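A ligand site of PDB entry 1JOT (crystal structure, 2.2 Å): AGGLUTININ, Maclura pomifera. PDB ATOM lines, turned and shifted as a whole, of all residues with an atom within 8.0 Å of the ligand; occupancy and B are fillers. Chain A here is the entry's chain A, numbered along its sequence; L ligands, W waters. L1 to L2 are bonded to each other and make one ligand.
Merely in contact with the ligand: Phe 47 (3.5 Å), Tyr 78 (2.9 Å) and Gly 121 (3.7 Å).
Hydrophobic or aromatic side chains that line the ligand: Phe 47, Tyr 78, Tyr 122 and Trp 123.
Of the 23 residues printed, 7 come within 4 Å of the ligand.
Water W1 lies within hydrogen-bond range of the backbone NH of Thr 79 (3.0 Å) and an oxygen (O5) of LG2 L2 (3.1 Å).
N of Gly 1 lies within hydrogen-bond range of O3 of LIG L1.
The side-chain carboxylate of Asp 125 sits at hydrogen-bond distance from an oxygen (O4) of LIG L1 (2.8 Å).
O5 of LIG L1 sits at hydrogen-bond distance from O of Trp 123, 3.4 Å away.
An oxygen (O5) of LIG L1 lies within hydrogen-bond range of the backbone NH of Tyr 122 (3.0 Å).
The backbone NH (N) of Trp 123 lies within hydrogen-bond range of an oxygen (O5) of LIG L1 (3.1 Å).
OD2 of Asp 125 lies within hydrogen-bond range of N of Gly 121 (3.4 Å).
N of Gly 1 lies close to OD2 of Asp 125, at 3.4 Å.
O of Tyr 122 sits at hydrogen-bond distance from OG of Ser 46, 2.6 Å away.
O of Gly 121 sits at hydrogen-bond distance from N of Phe 47, 2.6 Å away.
OG of Ser 119 sits at hydrogen-bond distance from OD2 of Asp 125, at 2.6 Å.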
ATOM      1  N   GLY A   1     -23.325  22.697  -3.361  1.00  0.00           N
ATOM      2  CA  GLY A   1     -24.296  23.423  -4.236  1.00  0.00           C
ATOM      3  C   GLY A   1     -23.604  24.420  -5.152  1.00  0.00           C
ATOM      4  O   GLY A   1     -22.388  24.523  -5.141  1.00  0.00           O
ATOM      5  N   VAL A   2     -24.391  25.136  -5.938  1.00  0.00           N
ATOM      6  CA  VAL A   2     -23.847  26.137  -6.850  1.00  0.00           C
ATOM      7  C   VAL A   2     -23.859  27.479  -6.137  1.00  0.00           C
ATOM      8  O   VAL A   2     -24.901  27.941  -5.659  1.00  0.00           O
ATOM      9  CB  VAL A   2     -24.696  26.224  -8.144  1.00  0.00           C
ATOM     10  CG1 VAL A   2     -24.327  27.458  -8.956  1.00  0.00           C
ATOM     11  CG2 VAL A   2     -24.468  24.979  -8.975  1.00  0.00           C
ATOM     12  N   THR A   3     -22.702  28.107  -6.042  1.00  0.00           N
ATOM     13  CA  THR A   3     -22.620  29.383  -5.362  1.00  0.00           C
ATOM     14  C   THR A   3     -23.185  30.514  -6.222  1.00  0.00           C
ATOM     15  O   THR A   3     -23.170  30.455  -7.457  1.00  0.00           O
ATOM     16  CB  THR A   3     -21.176  29.713  -4.988  1.00  0.00           C
ATOM     17  OG1 THR A   3     -20.420  29.905  -6.185  1.00  0.00           O
ATOM     18  CG2 THR A   3     -20.572  28.574  -4.180  1.00  0.00           C
ATOM     19  N   ALA A  24     -35.950  21.408   4.210  1.00  0.00           N
ATOM     20  CA  ALA A  24     -35.305  22.702   4.421  1.00  0.00           C
ATOM     21  C   ALA A  24     -35.683  23.721   3.366  1.00  0.00           C
ATOM     22  O   ALA A  24     -36.623  23.530   2.587  1.00  0.00           O
ATOM     23  CB  ALA A  24     -33.789  22.496   4.419  1.00  0.00           C
ATOM     24  N   ILE A  25     -34.931  24.821   3.339  1.00  0.00           N
ATOM     25  CA  ILE A  25     -35.175  25.886   2.376  1.00  0.00           C
ATOM     26  C   ILE A  25     -34.594  25.489   1.013  1.00  0.00           C
ATOM     27  O   ILE A  25     -33.497  24.915   0.927  1.00  0.00           O
ATOM     28  CB  ILE A  25     -34.550  27.221   2.844  1.00  0.00           C
ATOM     29  CG1 ILE A  25     -35.175  27.664   4.174  1.00  0.00           C
ATOM     30  CG2 ILE A  25     -34.746  28.303   1.776  1.00  0.00           C
ATOM     31  CD1 ILE A  25     -36.644  28.054   4.086  1.00  0.00           C
ATOM     32  N   SER A  46     -33.153  25.098  -6.737  1.00  0.00           N
ATOM     33  CA  SER A  46     -32.775  23.894  -6.025  1.00  0.00           C
ATOM     34  C   SER A  46     -32.485  22.816  -7.067  1.00  0.00           C
ATOM     35  O   SER A  46     -32.984  22.896  -8.190  1.00  0.00           O
ATOM     36  CB  SER A  46     -33.945  23.449  -5.143  1.00  0.00           C
ATOM     37  OG  SER A  46     -33.809  22.112  -4.730  1.00  0.00           O
ATOM     38  N   PHE A  47     -31.696  21.808  -6.700  1.00  0.00           N
ATOM     39  CA  PHE A  47     -31.372  20.728  -7.626  1.00  0.00           C
ATOM     40  C   PHE A  47     -32.567  19.780  -7.747  1.00  0.00           C
ATOM     41  O   PHE A  47     -32.581  18.920  -8.627  1.00  0.00           O
ATOM     42  CB  PHE A  47     -30.175  19.910  -7.131  1.00  0.00           C
ATOM     43  CG  PHE A  47     -28.849  20.602  -7.295  1.00  0.00           C
ATOM     44  CD1 PHE A  47     -28.760  21.888  -7.803  1.00  0.00           C
ATOM     45  CD2 PHE A  47     -27.674  19.969  -6.891  1.00  0.00           C
ATOM     46  CE1 PHE A  47     -27.525  22.534  -7.913  1.00  0.00           C
ATOM     47  CE2 PHE A  47     -26.437  20.600  -7.007  1.00  0.00           C
ATOM     48  CZ  PHE A  47     -26.364  21.878  -7.515  1.00  0.00           C
ATOM     49  N   ILE A  48     -33.544  19.916  -6.863  1.00  0.00           N
ATOM     50  CA  ILE A  48     -34.727  19.053  -6.857  1.00  0.00           C
ATOM     51  C   ILE A  48     -36.038  19.822  -6.815  1.00  0.00           C
ATOM     52  O   ILE A  48     -36.066  21.049  -6.863  1.00  0.00           O
ATOM     53  CB  ILE A  48     -34.696  18.096  -5.660  1.00  0.00           C
ATOM     54  CG1 ILE A  48     -34.471  18.878  -4.362  1.00  0.00           C
ATOM     55  CG2 ILE A  48     -33.618  17.061  -5.853  1.00  0.00           C
ATOM     56  CD1 ILE A  48     -34.552  18.037  -3.120  1.00  0.00           C
ATOM     57  N   VAL A  75     -29.676  17.821   7.034  1.00  0.00           N
ATOM     58  CA  VAL A  75     -30.679  17.085   6.267  1.00  0.00           C
ATOM     59  C   VAL A  75     -29.881  16.158   5.366  1.00  0.00           C
ATOM     60  O   VAL A  75     -29.036  16.596   4.584  1.00  0.00           O
ATOM     61  CB  VAL A  75     -31.573  18.015   5.409  1.00  0.00           C
ATOM     62  CG1 VAL A  75     -32.432  17.178   4.477  1.00  0.00           C
ATOM     63  CG2 VAL A  75     -32.466  18.858   6.299  1.00  0.00           C
ATOM     64  N   GLU A  76     -30.126  14.855   5.493  1.00  0.00           N
ATOM     65  CA  GLU A  76     -29.409  13.873   4.694  1.00  0.00           C
ATOM     66  C   GLU A  76     -27.905  14.079   4.860  1.00  0.00           C
ATOM     67  O   GLU A  76     -27.132  13.867   3.933  1.00  0.00           O
ATOM     68  CB  GLU A  76     -29.796  13.983   3.222  1.00  0.00           C
ATOM     69  CG  GLU A  76     -31.196  13.451   2.923  1.00  0.00           C
ATOM     70  CD  GLU A  76     -31.291  11.924   2.971  1.00  0.00           C
ATOM     71  OE1 GLU A  76     -30.254  11.243   3.154  1.00  0.00           O
ATOM     72  OE2 GLU A  76     -32.423  11.399   2.818  1.00  0.00           O
ATOM     73  N   GLY A  77     -27.512  14.532   6.053  1.00  0.00           N
ATOM     74  CA  GLY A  77     -26.104  14.752   6.347  1.00  0.00           C
ATOM     75  C   GLY A  77     -25.516  16.089   5.932  1.00  0.00           C
ATOM     76  O   GLY A  77     -24.348  16.365   6.219  1.00  0.00           O
ATOM     77  N   TYR A  78     -26.306  16.911   5.259  1.00  0.00           N
ATOM     78  CA  TYR A  78     -25.831  18.207   4.811  1.00  0.00           C
ATOM     79  C   TYR A  78     -26.310  19.293   5.756  1.00  0.00           C
ATOM     80  O   TYR A  78     -27.460  19.254   6.213  1.00  0.00           O
ATOM     81  CB  TYR A  78     -26.350  18.504   3.389  1.00  0.00           C
ATOM     82  CG  TYR A  78     -25.671  17.693   2.308  1.00  0.00           C
ATOM     83  CD1 TYR A  78     -24.334  17.903   1.981  1.00  0.00           C
ATOM     84  CD2 TYR A  78     -26.366  16.701   1.621  1.00  0.00           C
ATOM     85  CE1 TYR A  78     -23.707  17.137   1.005  1.00  0.00           C
ATOM     86  CE2 TYR A  78     -25.751  15.936   0.639  1.00  0.00           C
ATOM     87  CZ  TYR A  78     -24.418  16.166   0.342  1.00  0.00           C
ATOM     88  OH  TYR A  78     -23.810  15.401  -0.625  1.00  0.00           O
ATOM     89  N   THR A  79     -25.441  20.250   6.066  1.00  0.00           N
ATOM     90  CA  THR A  79     -25.808  21.359   6.954  1.00  0.00           C
ATOM     91  C   THR A  79     -26.422  22.443   6.090  1.00  0.00           C
ATOM     92  O   THR A  79     -25.738  23.044   5.262  1.00  0.00           O
ATOM     93  CB  THR A  79     -24.576  21.935   7.671  1.00  0.00           C
ATOM     94  OG1 THR A  79     -23.834  20.864   8.269  1.00  0.00           O
ATOM     95  CG2 THR A  79     -25.007  22.926   8.750  1.00  0.00           C
ATOM     96  N   VAL A  80     -27.703  22.697   6.287  1.00  0.00           N
ATOM     97  CA  VAL A  80     -28.395  23.695   5.477  1.00  0.00           C
ATOM     98  C   VAL A  80     -29.332  24.588   6.283  1.00  0.00           C
ATOM     99  O   VAL A  80     -29.585  24.341   7.459  1.00  0.00           O
ATOM    100  CB  VAL A  80     -29.223  22.988   4.376  1.00  0.00           C
ATOM    101  CG1 VAL A  80     -28.334  22.048   3.567  1.00  0.00           C
ATOM    102  CG2 VAL A  80     -30.361  22.194   5.004  1.00  0.00           C
ATOM    103  N   ILE A  81     -29.836  25.630   5.633  1.00  0.00           N
ATOM    104  CA  ILE A  81     -30.769  26.533   6.277  1.00  0.00           C
ATOM    105  C   ILE A  81     -32.124  25.836   6.194  1.00  0.00           C
ATOM    106  O   ILE A  81     -32.661  25.646   5.108  1.00  0.00           O
ATOM    107  CB  ILE A  81     -30.839  27.874   5.527  1.00  0.00           C
ATOM    108  CG1 ILE A  81     -29.425  28.442   5.370  1.00  0.00           C
ATOM    109  CG2 ILE A  81     -31.758  28.848   6.254  1.00  0.00           C
ATOM    110  CD1 ILE A  81     -28.884  29.109   6.600  1.00  0.00           C
ATOM    111  N   SER A 119     -25.101  29.754  -1.386  1.00  0.00           N
ATOM    112  CA  SER A 119     -24.977  28.521  -2.156  1.00  0.00           C
ATOM    113  C   SER A 119     -26.213  27.665  -2.029  1.00  0.00           C
ATOM    114  O   SER A 119     -26.780  27.530  -0.930  1.00  0.00           O
ATOM    115  CB  SER A 119     -23.762  27.723  -1.678  1.00  0.00           C
ATOM    116  OG  SER A 119     -23.916  26.352  -1.992  1.00  0.00           O
ATOM    117  N   ILE A 120     -26.650  27.090  -3.147  1.00  0.00           N
ATOM    118  CA  ILE A 120     -27.821  26.219  -3.168  1.00  0.00           C
ATOM    119  C   ILE A 120     -27.551  24.949  -3.974  1.00  0.00           C
ATOM    120  O   ILE A 120     -27.038  25.010  -5.085  1.00  0.00           O
ATOM    121  CB  ILE A 120     -29.052  26.928  -3.781  1.00  0.00           C
ATOM    122  CG1 ILE A 120     -29.384  28.198  -2.990  1.00  0.00           C
ATOM    123  CG2 ILE A 120     -30.261  25.996  -3.744  1.00  0.00           C
ATOM    124  CD1 ILE A 120     -30.337  29.130  -3.698  1.00  0.00           C
ATOM    125  N   GLY A 121     -27.884  23.815  -3.379  1.00  0.00           N
ATOM    126  CA  GLY A 121     -27.737  22.520  -4.038  1.00  0.00           C
ATOM    127  C   GLY A 121     -29.158  21.970  -4.017  1.00  0.00           C
ATOM    128  O   GLY A 121     -30.010  22.435  -4.771  1.00  0.00           O
ATOM    129  N   TYR A 122     -29.412  21.005  -3.138  1.00  0.00           N
ATOM    130  CA  TYR A 122     -30.754  20.461  -2.981  1.00  0.00           C
ATOM    131  C   TYR A 122     -31.502  21.494  -2.138  1.00  0.00           C
ATOM    132  O   TYR A 122     -32.679  21.789  -2.375  1.00  0.00           O
ATOM    133  CB  TYR A 122     -30.714  19.131  -2.232  1.00  0.00           C
ATOM    134  CG  TYR A 122     -30.250  17.969  -3.088  1.00  0.00           C
ATOM    135  CD1 TYR A 122     -30.766  17.769  -4.361  1.00  0.00           C
ATOM    136  CD2 TYR A 122     -29.258  17.093  -2.629  1.00  0.00           C
ATOM    137  CE1 TYR A 122     -30.338  16.723  -5.151  1.00  0.00           C
ATOM    138  CE2 TYR A 122     -28.813  16.037  -3.424  1.00  0.00           C
ATOM    139  CZ  TYR A 122     -29.364  15.855  -4.687  1.00  0.00           C
ATOM    140  OH  TYR A 122     -28.942  14.825  -5.493  1.00  0.00           O
ATOM    141  N   TRP A 123     -30.782  22.048  -1.170  1.00  0.00           N
ATOM    142  CA  TRP A 123     -31.336  23.066  -0.279  1.00  0.00           C
ATOM    143  C   TRP A 123     -30.370  24.237  -0.146  1.00  0.00           C
ATOM    144  O   TRP A 123     -29.227  24.177  -0.607  1.00  0.00           O
ATOM    145  CB  TRP A 123     -31.613  22.445   1.092  1.00  0.00           C
ATOM    146  CG  TRP A 123     -32.449  21.208   1.005  1.00  0.00           C
ATOM    147  CD1 TRP A 123     -33.797  21.142   0.758  1.00  0.00           C
ATOM    148  CD2 TRP A 123     -31.987  19.849   1.088  1.00  0.00           C
ATOM    149  NE1 TRP A 123     -34.203  19.823   0.686  1.00  0.00           N
ATOM    150  CE2 TRP A 123     -33.113  19.011   0.886  1.00  0.00           C
ATOM    151  CE3 TRP A 123     -30.738  19.255   1.317  1.00  0.00           C
ATOM    152  CZ2 TRP A 123     -33.026  17.605   0.895  1.00  0.00           C
ATOM    153  CZ3 TRP A 123     -30.653  17.866   1.333  1.00  0.00           C
ATOM    154  CH2 TRP A 123     -31.787  17.060   1.120  1.00  0.00           C
ATOM    155  N   LEU A 124     -30.843  25.317   0.473  1.00  0.00           N
ATOM    156  CA  LEU A 124     -30.000  26.496   0.690  1.00  0.00           C
ATOM    157  C   LEU A 124     -28.872  26.072   1.632  1.00  0.00           C
ATOM    158  O   LEU A 124     -29.101  25.746   2.793  1.00  0.00           O
ATOM    159  CB  LEU A 124     -30.838  27.611   1.315  1.00  0.00           C
ATOM    160  CG  LEU A 124     -30.171  28.960   1.587  1.00  0.00           C
ATOM    161  CD1 LEU A 124     -29.699  29.578   0.285  1.00  0.00           C
ATOM    162  CD2 LEU A 124     -31.148  29.884   2.281  1.00  0.00           C
ATOM    163  N   ASP A 125     -27.639  26.058   1.117  1.00  0.00           N
ATOM    164  CA  ASP A 125     -26.504  25.639   1.910  1.00  0.00           C
ATOM    165  C   ASP A 125     -26.095  26.673   2.944  1.00  0.00           C
ATOM    166  O   ASP A 125     -25.871  26.355   4.119  1.00  0.00           O
ATOM    167  CB  ASP A 125     -25.318  25.339   0.998  1.00  0.00           C
ATOM    168  CG  ASP A 125     -25.585  24.173   0.090  1.00  0.00           C
ATOM    169  OD1 ASP A 125     -25.990  23.108   0.597  1.00  0.00           O
ATOM    170  OD2 ASP A 125     -25.386  24.323  -1.136  1.00  0.00           O
ATOM    171  N   TYR A 126     -26.009  27.916   2.504  1.00  0.00           N
ATOM    172  CA  TYR A 126     -25.625  29.010   3.382  1.00  0.00           C
ATOM    173  C   TYR A 126     -25.803  30.309   2.621  1.00  0.00           C
ATOM    174  O   TYR A 126     -25.885  30.310   1.387  1.00  0.00           O
ATOM    175  CB  TYR A 126     -24.165  28.838   3.804  1.00  0.00           C
ATOM    176  CG  TYR A 126     -23.196  28.765   2.656  1.00  0.00           C
ATOM    177  CD1 TYR A 126     -22.840  29.918   1.945  1.00  0.00           C
ATOM    178  CD2 TYR A 126     -22.610  27.546   2.278  1.00  0.00           C
ATOM    179  CE1 TYR A 126     -21.928  29.861   0.893  1.00  0.00           C
ATOM    180  CE2 TYR A 126     -21.701  27.481   1.231  1.00  0.00           C
ATOM    181  CZ  TYR A 126     -21.360  28.639   0.538  1.00  0.00           C
ATOM    182  OH  TYR A 126     -20.429  28.592  -0.468  1.00  0.00           O
HETATM  183  O1  LIG L   1     -26.883  19.376  -2.220  1.00  0.00           O
HETATM  184  C1  LIG L   1     -26.110  18.684  -3.232  1.00  0.00           C
HETATM  185  O2  LIG L   1     -25.886  17.361  -2.787  1.00  0.00           O
HETATM  186  C2  LIG L   1     -24.764  19.381  -3.457  1.00  0.00           C
HETATM  187  N1  LIG L   1     -23.985  18.630  -4.422  1.00  0.00           N
HETATM  188  C3  LIG L   1     -24.000  19.490  -2.130  1.00  0.00           C
HETATM  189  O3  LIG L   1     -22.799  20.253  -2.331  1.00  0.00           O
HETATM  190  C4  LIG L   1     -24.879  20.188  -1.090  1.00  0.00           C
HETATM  191  O4  LIG L   1     -25.124  21.517  -1.539  1.00  0.00           O
HETATM  192  C5  LIG L   1     -26.207  19.435  -0.947  1.00  0.00           C
HETATM  193  C6  LIG L   1     -27.107  20.122   0.084  1.00  0.00           C
HETATM  194  O5  LIG L   1     -27.915  21.093  -0.558  1.00  0.00           O
HETATM  195  C7  LIG L   1     -23.314  19.261  -5.388  1.00  0.00           C
HETATM  196  O6  LIG L   1     -23.315  20.477  -5.519  1.00  0.00           O
HETATM  197  C8  LIG L   1     -22.531  18.391  -6.366  1.00  0.00           C
HETATM  198  C1  LG2 L   2     -21.631  19.585  -1.848  1.00  0.00           C
HETATM  199  C2  LG2 L   2     -20.396  20.146  -2.561  1.00  0.00           C
HETATM  200  C3  LG2 L   2     -19.086  19.601  -1.975  1.00  0.00           C
HETATM  201  C4  LG2 L   2     -19.088  19.727  -0.461  1.00  0.00           C
HETATM  202  C5  LG2 L   2     -20.340  19.077   0.116  1.00  0.00           C
HETATM  203  C6  LG2 L   2     -20.321  19.169   1.645  1.00  0.00           C
HETATM  204  O1  LG2 L   2     -20.463  19.795  -3.942  1.00  0.00           O
HETATM  205  O2  LG2 L   2     -17.996  20.337  -2.504  1.00  0.00           O
HETATM  206  O3  LG2 L   2     -19.060  21.105  -0.109  1.00  0.00           O
HETATM  207  O4  LG2 L   2     -21.511  19.743  -0.412  1.00  0.00           O
HETATM  208  O5  LG2 L   2     -21.637  19.074   2.153  1.00  0.00           O
HETATM  209  O   HOH W   1     -22.910  20.543   4.516  1.00  0.00           O
